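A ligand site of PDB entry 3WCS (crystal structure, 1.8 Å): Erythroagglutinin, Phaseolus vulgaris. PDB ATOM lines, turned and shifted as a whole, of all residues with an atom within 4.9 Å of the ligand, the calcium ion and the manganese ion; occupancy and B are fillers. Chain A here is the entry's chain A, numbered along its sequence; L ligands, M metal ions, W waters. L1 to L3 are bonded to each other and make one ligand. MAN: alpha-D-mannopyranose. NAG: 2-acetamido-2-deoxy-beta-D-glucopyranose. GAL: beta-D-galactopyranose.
Water W3 lies within hydrogen-bond range of OE1 of Glu 124 (2.7 Å), O of Ile 147 (3.1 Å) and NE1 of Trp 133 (3.4 Å). Water W13 lies within hydrogen-bond range of an oxygen (O3) of NAG L2 (2.7 Å), the backbone carbonyl oxygen of Tyr 129 (2.7 Å) and the backbone NH of Val 131 (3.0 Å). Water W14 lies within hydrogen-bond range of OD1 of Asp 86, ND2 of Asn 130, O3 of MAN L1 and N of Gly 104. Water W2 lies within hydrogen-bond range of O7 of NAG L2 (2.7 Å), N of His 132 (2.9 Å) and N of Val 131 (3.4 Å). Water W8 lies within hydrogen-bond range of an oxygen (O6) of GAL L3 (2.7 Å) and the backbone NH (N) of Tyr 129 (2.9 Å). Water W12 lies within hydrogen-bond range of an oxygen (O6) of NAG L2, the side-chain carboxylate of Asp 86 and the backbone NH of Ile 215.
The manganese ion is bound by water W3, water W7, OD1 of Asp 134, NE2 of His 139, OE2 of Glu 124 and OD2 of Asp 126.
The side-chain amide nitrogen (ND2) of Asn 219 sits at hydrogen-bond distance from the backbone carbonyl oxygen (O) of Thr 216. The backbone carbonyl oxygen of Asn 219 lies close to the backbone NH of Gly 214, at 3.2 Å. The side-chain carboxylate of Asp 134 sits close to the indole nitrogen of Trp 133 (3.4 Å). The side-chain carboxylate of Asp 86 sits close to the backbone NH of Gly 104, 3.5 Å away.
Gly 103 touches the ligand. N of Leu 105 touches O4 of MAN L1, at 3.6 Å. O of Tyr 129 touches C6 of GAL L3, at 3.7 Å. Val 131 touches the ligand. His 132 touches the ligand. CH2 of Trp 133 touches C6 of MAN L1 (3.7 Å). CA of Gly 214 touches O6 of NAG L2, 3.8 Å away. Within 4 Å of the ligand: Gly 103, Gly 104, Leu 105, Leu 128, Tyr 129, Asn 130, Val 131, His 132, Trp 133, Gly 214, Ile 215, Thr 216 and Asn 219. Along chain A the residues within 4 Å of the ligand span positions 103 to 219. The nearest printed residue that does not touch the ligand is Lys 102 (4.05 Å).
Water W10 is bound to the calcium ion, at 2.3 Å. The side-chain carboxylate (OD2) of Asp 134 binds the calcium ion (2.3 Å). Water W1 binds the calcium ion, 2.3 Å away. The side-chain carboxylate (OD1) of Asp 126 binds the calcium ion, at 2.3 Å. The calcium ion is bound by the side-chain amide oxygen (OD1) of Asn 130 (2.3 Å). O of Leu 128 is bound to the calcium ion (2.4 Å). OD2 of Asp 126 is bound to the calcium ion.
Four residues have an atom within 4 Å of the manganese ion: Glu 124, Asp 126, Asp 134 and His 139. The nearest printed residue that does not touch the manganese ion is Ser 149 (4.3 Å).
Within 4 Å of the calcium ion: Asp 126, Leu 128, Asn 130 and Asp 134. The nearest printed residue that does not touch the calcium ion is Trp 133 (4.3 Å).
An oxygen (O6) of NAG L2 sits at hydrogen-bond distance from the backbone NH (N) of Ile 215, at 3.2 Å. N of Thr 216 is in hydrogen-bond range of O6 of NAG L2 (3.2 Å). N of Gly 104 sits at hydrogen-bond distance from O3 of MAN L1, at 2.8 Å. OG1 of Thr 216 lies within hydrogen-bond range of O6 of NAG L2. O7 of NAG L2 sits at hydrogen-bond distance from ND2 of Asn 130. The side-chain amide nitrogen (ND2) of Asn 219 is in hydrogen-bond range of an oxygen (O2) of GAL L3 (3.0 Å).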
ATOM      1  N   ASP A  86       2.621  -3.885   4.638  1.00  0.00           N
ATOM      2  CA  ASP A  86       3.794  -2.969   4.604  1.00  0.00           C
ATOM      3  C   ASP A  86       4.614  -3.165   3.341  1.00  0.00           C
ATOM      4  O   ASP A  86       5.436  -2.300   2.966  1.00  0.00           O
ATOM      5  CB  ASP A  86       4.699  -3.263   5.803  1.00  0.00           C
ATOM      6  CG  ASP A  86       4.382  -2.406   6.984  1.00  0.00           C
ATOM      7  OD1 ASP A  86       4.791  -1.211   6.964  1.00  0.00           O
ATOM      8  OD2 ASP A  86       3.775  -2.917   7.958  1.00  0.00           O
ATOM      9  N   LYS A 102       8.764  -7.446  12.435  1.00  0.00           N
ATOM     10  CA  LYS A 102       7.648  -7.345  11.496  1.00  0.00           C
ATOM     11  C   LYS A 102       7.346  -5.907  11.049  1.00  0.00           C
ATOM     12  O   LYS A 102       8.180  -4.992  11.194  1.00  0.00           O
ATOM     13  CB  LYS A 102       6.407  -8.005  12.111  1.00  0.00           C
ATOM     14  CG  LYS A 102       5.882  -7.300  13.365  1.00  0.00           C
ATOM     15  CD  LYS A 102       4.582  -7.930  13.871  1.00  0.00           C
ATOM     16  CE  LYS A 102       4.854  -9.083  14.826  1.00  0.00           C
ATOM     17  NZ  LYS A 102       3.593  -9.805  15.164  1.00  0.00           N
ATOM     18  N   GLY A 103       6.164  -5.708  10.473  1.00  0.00           N
ATOM     19  CA  GLY A 103       5.768  -4.363  10.018  1.00  0.00           C
ATOM     20  C   GLY A 103       6.728  -3.752   8.994  1.00  0.00           C
ATOM     21  O   GLY A 103       7.143  -4.396   8.039  1.00  0.00           O
ATOM     22  N   GLY A 104       7.108  -2.486   9.229  1.00  0.00           N
ATOM     23  CA  GLY A 104       7.936  -1.777   8.265  1.00  0.00           C
ATOM     24  C   GLY A 104       9.358  -2.326   8.109  1.00  0.00           C
ATOM     25  O   GLY A 104      10.069  -1.956   7.206  1.00  0.00           O
ATOM     26  N   LEU A 105       9.773  -3.191   9.011  1.00  0.00           N
ATOM     27  CA  LEU A 105      11.096  -3.789   8.900  1.00  0.00           C
ATOM     28  C   LEU A 105      11.084  -5.069   8.038  1.00  0.00           C
ATOM     29  O   LEU A 105      12.140  -5.674   7.788  1.00  0.00           O
ATOM     30  CB  LEU A 105      11.659  -4.044  10.300  1.00  0.00           C
ATOM     31  CG  LEU A 105      11.864  -2.743  11.115  1.00  0.00           C
ATOM     32  CD1 LEU A 105      12.234  -3.036  12.567  1.00  0.00           C
ATOM     33  CD2 LEU A 105      12.864  -1.810  10.445  1.00  0.00           C
ATOM     34  N   TYR A 112      16.168   0.288  12.284  1.00  0.00           N
ATOM     35  CA  TYR A 112      16.425   0.933  10.995  1.00  0.00           C
ATOM     36  C   TYR A 112      17.853   1.463  10.801  1.00  0.00           C
ATOM     37  O   TYR A 112      18.092   2.298   9.934  1.00  0.00           O
ATOM     38  CB  TYR A 112      15.371   2.000  10.673  1.00  0.00           C
ATOM     39  CG  TYR A 112      15.120   3.072  11.727  1.00  0.00           C
ATOM     40  CD1 TYR A 112      15.791   4.300  11.687  1.00  0.00           C
ATOM     41  CD2 TYR A 112      14.165   2.878  12.725  1.00  0.00           C
ATOM     42  CE1 TYR A 112      15.538   5.295  12.637  1.00  0.00           C
ATOM     43  CE2 TYR A 112      13.891   3.865  13.673  1.00  0.00           C
ATOM     44  CZ  TYR A 112      14.586   5.060  13.626  1.00  0.00           C
ATOM     45  OH  TYR A 112      14.285   6.015  14.574  1.00  0.00           O
ATOM     46  N   GLU A 124      12.918  -4.393  -2.434  1.00  0.00           N
ATOM     47  CA  GLU A 124      11.658  -4.184  -1.728  1.00  0.00           C
ATOM     48  C   GLU A 124      10.616  -3.456  -2.552  1.00  0.00           C
ATOM     49  O   GLU A 124      10.946  -2.624  -3.405  1.00  0.00           O
ATOM     50  CB  GLU A 124      11.865  -3.438  -0.406  1.00  0.00           C
ATOM     51  CG  GLU A 124      12.416  -1.999  -0.562  1.00  0.00           C
ATOM     52  CD  GLU A 124      12.272  -1.160   0.715  1.00  0.00           C
ATOM     53  OE1 GLU A 124      12.759  -1.655   1.769  1.00  0.00           O
ATOM     54  OE2 GLU A 124      11.682  -0.028   0.712  1.00  0.00           O
ATOM     55  N   ASP A 126       7.620  -1.458  -1.455  1.00  0.00           N
ATOM     56  CA  ASP A 126       7.261  -0.868  -0.129  1.00  0.00           C
ATOM     57  C   ASP A 126       6.004  -0.008  -0.308  1.00  0.00           C
ATOM     58  O   ASP A 126       6.007   0.964  -1.069  1.00  0.00           O
ATOM     59  CB  ASP A 126       8.474  -0.030   0.377  1.00  0.00           C
ATOM     60  CG  ASP A 126       8.339   0.471   1.836  1.00  0.00           C
ATOM     61  OD1 ASP A 126       7.208   0.415   2.355  1.00  0.00           O
ATOM     62  OD2 ASP A 126       9.384   0.912   2.468  1.00  0.00           O
ATOM     63  N   LEU A 128       4.134   1.342   2.320  1.00  0.00           N
ATOM     64  CA  LEU A 128       3.834   2.155   3.511  1.00  0.00           C
ATOM     65  C   LEU A 128       5.018   3.055   3.856  1.00  0.00           C
ATOM     66  O   LEU A 128       6.124   2.594   4.111  1.00  0.00           O
ATOM     67  CB  LEU A 128       3.477   1.269   4.711  1.00  0.00           C
ATOM     68  CG  LEU A 128       2.994   2.260   5.804  1.00  0.00           C
ATOM     69  CD1 LEU A 128       1.531   2.160   6.223  1.00  0.00           C
ATOM     70  CD2 LEU A 128       4.015   2.462   6.931  1.00  0.00           C
ATOM     71  N   TYR A 129       4.735   4.358   3.882  1.00  0.00           N
ATOM     72  CA  TYR A 129       5.762   5.364   4.247  1.00  0.00           C
ATOM     73  C   TYR A 129       6.115   5.312   5.730  1.00  0.00           C
ATOM     74  O   TYR A 129       5.266   5.601   6.591  1.00  0.00           O
ATOM     75  CB  TYR A 129       5.211   6.727   3.871  1.00  0.00           C
ATOM     76  CG  TYR A 129       5.917   7.924   4.508  1.00  0.00           C
ATOM     77  CD1 TYR A 129       7.259   8.134   4.308  1.00  0.00           C
ATOM     78  CD2 TYR A 129       5.219   8.791   5.331  1.00  0.00           C
ATOM     79  CE1 TYR A 129       7.889   9.250   4.889  1.00  0.00           C
ATOM     80  CE2 TYR A 129       5.828   9.897   5.918  1.00  0.00           C
ATOM     81  CZ  TYR A 129       7.157  10.111   5.699  1.00  0.00           C
ATOM     82  OH  TYR A 129       7.757  11.221   6.297  1.00  0.00           O
ATOM     83  N   ASN A 130       7.368   4.954   6.030  1.00  0.00           N
ATOM     84  CA  ASN A 130       7.829   4.865   7.405  1.00  0.00           C
ATOM     85  C   ASN A 130       8.667   6.115   7.618  1.00  0.00           C
ATOM     86  O   ASN A 130       9.725   6.270   7.028  1.00  0.00           O
ATOM     87  CB  ASN A 130       8.655   3.591   7.631  1.00  0.00           C
ATOM     88  CG  ASN A 130       7.785   2.341   7.697  1.00  0.00           C
ATOM     89  OD1 ASN A 130       7.721   1.551   6.732  1.00  0.00           O
ATOM     90  ND2 ASN A 130       7.124   2.154   8.846  1.00  0.00           N
ATOM     91  N   VAL A 131       8.144   7.019   8.438  1.00  0.00           N
ATOM     92  CA  VAL A 131       8.703   8.377   8.571  1.00  0.00           C
ATOM     93  C   VAL A 131      10.198   8.468   8.855  1.00  0.00           C
ATOM     94  O   VAL A 131      10.869   9.416   8.422  1.00  0.00           O
ATOM     95  CB  VAL A 131       7.880   9.175   9.628  1.00  0.00           C
ATOM     96  CG1 VAL A 131       7.992   8.543  11.011  1.00  0.00           C
ATOM     97  CG2 VAL A 131       8.297  10.636   9.658  1.00  0.00           C
ATOM     98  N   HIS A 132      10.737   7.493   9.569  1.00  0.00           N
ATOM     99  CA  HIS A 132      12.145   7.575  10.002  1.00  0.00           C
ATOM    100  C   HIS A 132      13.162   7.175   8.965  1.00  0.00           C
ATOM    101  O   HIS A 132      14.372   7.388   9.142  1.00  0.00           O
ATOM    102  CB  HIS A 132      12.364   6.804  11.301  1.00  0.00           C
ATOM    103  CG  HIS A 132      11.538   7.312  12.459  1.00  0.00           C
ATOM    104  ND1 HIS A 132      11.599   8.595  12.900  1.00  0.00           N
ATOM    105  CD2 HIS A 132      10.658   6.641  13.316  1.00  0.00           C
ATOM    106  CE1 HIS A 132      10.767   8.758  13.946  1.00  0.00           C
ATOM    107  NE2 HIS A 132      10.186   7.559  14.215  1.00  0.00           N
ATOM    108  N   TRP A 133      12.712   6.585   7.847  1.00  0.00           N
ATOM    109  CA  TRP A 133      13.646   6.153   6.798  1.00  0.00           C
ATOM    110  C   TRP A 133      13.207   6.174   5.354  1.00  0.00           C
ATOM    111  O   TRP A 133      14.037   6.210   4.473  1.00  0.00           O
ATOM    112  CB  TRP A 133      14.236   4.779   7.141  1.00  0.00           C
ATOM    113  CG  TRP A 133      13.210   3.668   7.070  1.00  0.00           C
ATOM    114  CD1 TRP A 133      12.773   3.002   5.933  1.00  0.00           C
ATOM    115  CD2 TRP A 133      12.523   3.034   8.184  1.00  0.00           C
ATOM    116  NE1 TRP A 133      11.832   2.036   6.266  1.00  0.00           N
ATOM    117  CE2 TRP A 133      11.654   1.994   7.601  1.00  0.00           C
ATOM    118  CE3 TRP A 133      12.505   3.219   9.567  1.00  0.00           C
ATOM    119  CZ2 TRP A 133      10.844   1.202   8.379  1.00  0.00           C
ATOM    120  CZ3 TRP A 133      11.682   2.413  10.340  1.00  0.00           C
ATOM    121  CH2 TRP A 133      10.859   1.429   9.753  1.00  0.00           C
ATOM    122  N   ASP A 134      11.902   6.102   5.084  1.00  0.00           N
ATOM    123  CA  ASP A 134      11.403   5.991   3.706  1.00  0.00           C
ATOM    124  C   ASP A 134      11.202   7.337   2.992  1.00  0.00           C
ATOM    125  O   ASP A 134      10.856   8.314   3.644  1.00  0.00           O
ATOM    126  CB  ASP A 134      10.027   5.295   3.705  1.00  0.00           C
ATOM    127  CG  ASP A 134      10.122   3.756   3.743  1.00  0.00           C
ATOM    128  OD1 ASP A 134      11.060   3.126   3.149  1.00  0.00           O
ATOM    129  OD2 ASP A 134       9.161   3.183   4.332  1.00  0.00           O
ATOM    130  N   PRO A 135      11.333   7.359   1.638  1.00  0.00           N
ATOM    131  CA  PRO A 135      10.757   8.434   0.835  1.00  0.00           C
ATOM    132  C   PRO A 135       9.234   8.352   0.966  1.00  0.00           C
ATOM    133  O   PRO A 135       8.696   7.271   1.216  1.00  0.00           O
ATOM    134  CB  PRO A 135      11.205   8.112  -0.593  1.00  0.00           C
ATOM    135  CG  PRO A 135      11.483   6.642  -0.600  1.00  0.00           C
ATOM    136  CD  PRO A 135      11.863   6.248   0.796  1.00  0.00           C
ATOM    137  N   HIS A 139       7.381   2.906  -3.298  1.00  0.00           N
ATOM    138  CA  HIS A 139       8.667   2.819  -3.982  1.00  0.00           C
ATOM    139  C   HIS A 139       9.163   1.403  -4.130  1.00  0.00           C
ATOM    140  O   HIS A 139       8.786   0.501  -3.359  1.00  0.00           O
ATOM    141  CB  HIS A 139       9.727   3.677  -3.229  1.00  0.00           C
ATOM    142  CG  HIS A 139       9.863   3.367  -1.752  1.00  0.00           C
ATOM    143  ND1 HIS A 139       9.030   3.881  -0.821  1.00  0.00           N
ATOM    144  CD2 HIS A 139      10.745   2.509  -1.073  1.00  0.00           C
ATOM    145  CE1 HIS A 139       9.391   3.420   0.401  1.00  0.00           C
ATOM    146  NE2 HIS A 139      10.442   2.553   0.258  1.00  0.00           N
ATOM    147  N   ILE A 147      17.176  -1.378   6.229  1.00  0.00           N
ATOM    148  CA  ILE A 147      15.839  -1.031   5.716  1.00  0.00           C
ATOM    149  C   ILE A 147      15.864   0.332   5.007  1.00  0.00           C
ATOM    150  O   ILE A 147      14.956   0.661   4.241  1.00  0.00           O
ATOM    151  CB  ILE A 147      14.748  -1.093   6.815  1.00  0.00           C
ATOM    152  CG1 ILE A 147      13.340  -1.204   6.209  1.00  0.00           C
ATOM    153  CG2 ILE A 147      14.796   0.164   7.693  1.00  0.00           C
ATOM    154  CD1 ILE A 147      13.051  -2.533   5.507  1.00  0.00           C
ATOM    155  N   SER A 149      16.901   2.099   2.125  1.00  0.00           N
ATOM    156  CA  SER A 149      17.360   1.612   0.800  1.00  0.00           C
ATOM    157  C   SER A 149      18.527   2.426   0.305  1.00  0.00           C
ATOM    158  O   SER A 149      18.524   3.639   0.486  1.00  0.00           O
ATOM    159  CB  SER A 149      16.236   1.705  -0.225  1.00  0.00           C
ATOM    160  OG  SER A 149      15.117   0.957   0.229  1.00  0.00           O
ATOM    161  N   GLY A 214       0.541  -4.443   7.959  1.00  0.00           N
ATOM    162  CA  GLY A 214       0.615  -3.341   8.912  1.00  0.00           C
ATOM    163  C   GLY A 214       0.266  -3.789  10.320  1.00  0.00           C
ATOM    164  O   GLY A 214      -0.495  -4.748  10.508  1.00  0.00           O
ATOM    165  N   ILE A 215       0.819  -3.114  11.310  1.00  0.00           N
ATOM    166  CA  ILE A 215       0.508  -3.464  12.693  1.00  0.00           C
ATOM    167  C   ILE A 215      -0.685  -2.676  13.243  1.00  0.00           C
ATOM    168  O   ILE A 215      -1.236  -3.024  14.283  1.00  0.00           O
ATOM    169  CB  ILE A 215       1.733  -3.372  13.626  1.00  0.00           C
ATOM    170  CG1 ILE A 215       2.243  -1.916  13.762  1.00  0.00           C
ATOM    171  CG2 ILE A 215       2.852  -4.276  13.135  1.00  0.00           C
ATOM    172  CD1 ILE A 215       3.205  -1.727  14.924  1.00  0.00           C
ATOM    173  N   THR A 216      -1.081  -1.623  12.525  1.00  0.00           N
ATOM    174  CA  THR A 216      -2.140  -0.713  12.958  1.00  0.00           C
ATOM    175  C   THR A 216      -3.364  -0.859  12.063  1.00  0.00           C
ATOM    176  O   THR A 216      -3.242  -0.825  10.826  1.00  0.00           O
ATOM    177  CB  THR A 216      -1.659   0.750  12.888  1.00  0.00           C
ATOM    178  OG1 THR A 216      -0.502   0.893  13.717  1.00  0.00           O
ATOM    179  CG2 THR A 216      -2.738   1.705  13.363  1.00  0.00           C
ATOM    180  N   ASN A 219      -4.193  -0.432   7.860  1.00  0.00           N
ATOM    181  CA  ASN A 219      -2.972  -0.588   7.052  1.00  0.00           C
ATOM    182  C   ASN A 219      -2.684  -2.080   6.905  1.00  0.00           C
ATOM    183  O   ASN A 219      -2.106  -2.699   7.786  1.00  0.00           O
ATOM    184  CB  ASN A 219      -1.775   0.085   7.742  1.00  0.00           C
ATOM    185  CG  ASN A 219      -2.045   1.549   8.059  1.00  0.00           C
ATOM    186  OD1 ASN A 219      -1.844   2.413   7.208  1.00  0.00           O
ATOM    187  ND2 ASN A 219      -2.524   1.816   9.264  1.00  0.00           N
HETATM  188  C1  MAN L   1       6.055   1.262  14.179  1.00  0.00           C
HETATM  189  C2  MAN L   1       5.438   0.640  12.931  1.00  0.00           C
HETATM  190  C3  MAN L   1       6.338  -0.509  12.438  1.00  0.00           C
HETATM  191  C4  MAN L   1       7.737   0.024  12.139  1.00  0.00           C
HETATM  192  C5  MAN L   1       8.289   0.639  13.424  1.00  0.00           C
HETATM  193  C6  MAN L   1       9.689   1.225  13.263  1.00  0.00           C
HETATM  194  O1  MAN L   1       6.028   0.340  15.251  1.00  0.00           O
HETATM  195  O2  MAN L   1       5.396   1.598  11.896  1.00  0.00           O
HETATM  196  O3  MAN L   1       5.768  -1.042  11.257  1.00  0.00           O
HETATM  197  O4  MAN L   1       8.602  -0.993  11.637  1.00  0.00           O
HETATM  198  O5  MAN L   1       7.399   1.667  13.875  1.00  0.00           O
HETATM  199  O6  MAN L   1      10.202   1.543  14.551  1.00  0.00           O
HETATM  200  C1  NAG L   2       4.129   2.281  11.835  1.00  0.00           C
HETATM  201  C2  NAG L   2       4.402   3.687  11.295  1.00  0.00           C
HETATM  202  C3  NAG L   2       3.087   4.440  11.147  1.00  0.00           C
HETATM  203  C4  NAG L   2       2.061   3.652  10.332  1.00  0.00           C
HETATM  204  C5  NAG L   2       1.922   2.229  10.895  1.00  0.00           C
HETATM  205  C6  NAG L   2       1.049   1.337  10.019  1.00  0.00           C
HETATM  206  C7  NAG L   2       6.555   4.633  11.989  1.00  0.00           C
HETATM  207  C8  NAG L   2       7.296   5.355  13.084  1.00  0.00           C
HETATM  208  N2  NAG L   2       5.277   4.380  12.233  1.00  0.00           N
HETATM  209  O3  NAG L   2       3.323   5.701  10.556  1.00  0.00           O
HETATM  210  O4  NAG L   2       0.836   4.361  10.466  1.00  0.00           O
HETATM  211  O5  NAG L   2       3.197   1.610  10.993  1.00  0.00           O
HETATM  212  O6  NAG L   2       0.953   0.063  10.644  1.00  0.00           O
HETATM  213  O7  NAG L   2       7.141   4.302  10.949  1.00  0.00           O
HETATM  214  C1  GAL L   3       0.233   4.651   9.208  1.00  0.00           C
HETATM  215  C2  GAL L   3      -1.068   5.396   9.494  1.00  0.00           C
HETATM  216  C3  GAL L   3      -1.685   5.853   8.175  1.00  0.00           C
HETATM  217  C4  GAL L   3      -0.671   6.632   7.342  1.00  0.00           C
HETATM  218  C5  GAL L   3       0.615   5.820   7.142  1.00  0.00           C
HETATM  219  C6  GAL L   3       1.739   6.604   6.461  1.00  0.00           C
HETATM  220  O2  GAL L   3      -1.947   4.575  10.250  1.00  0.00           O
HETATM  221  O3  GAL L   3      -2.818   6.663   8.434  1.00  0.00           O
HETATM  222  O4  GAL L   3      -0.330   7.820   8.041  1.00  0.00           O
HETATM  223  O5  GAL L   3       1.095   5.444   8.413  1.00  0.00           O
HETATM  224  O6  GAL L   3       1.433   6.976   5.146  1.00  0.00           O
HETATM  225 CA    CA M   1       7.988   1.190   4.427  1.00  0.00          CA
HETATM  226 MN    MN M   2      11.214   1.580   1.864  1.00  0.00          MN
HETATM  227  O   HOH W   1       9.910  -0.019   4.972  1.00  0.00           O
HETATM  228  O   HOH W   2       9.744   4.995  10.659  1.00  0.00           O
HETATM  229  O   HOH W   3      12.041   0.438   3.231  1.00  0.00           O
HETATM  230  O   HOH W   4       8.579  -3.190  13.226  1.00  0.00           O
HETATM  231  O   HOH W   5       1.571   7.959  10.086  1.00  0.00           O
HETATM  232  O   HOH W   6      10.007   4.129  15.567  1.00  0.00           O
HETATM  233  O   HOH W   7      12.996   2.440   1.576  1.00  0.00           O
HETATM  234  O   HOH W   8       2.066   5.294   3.083  1.00  0.00           O
HETATM  235  O   HOH W   9      12.756   0.377  14.725  1.00  0.00           O
HETATM  236  O   HOH W  10       6.630  -0.638   4.793  1.00  0.00           O
HETATM  237  O   HOH W  11       4.093   5.305  14.650  1.00  0.00           O
HETATM  238  O   HOH W  12       3.097  -1.691  10.386  1.00  0.00           O
HETATM  239  O   HOH W  13       5.261   6.821   9.051  1.00  0.00           O
HETATM  240  O   HOH W  14       5.138   0.350   9.033  1.00  0.00           O
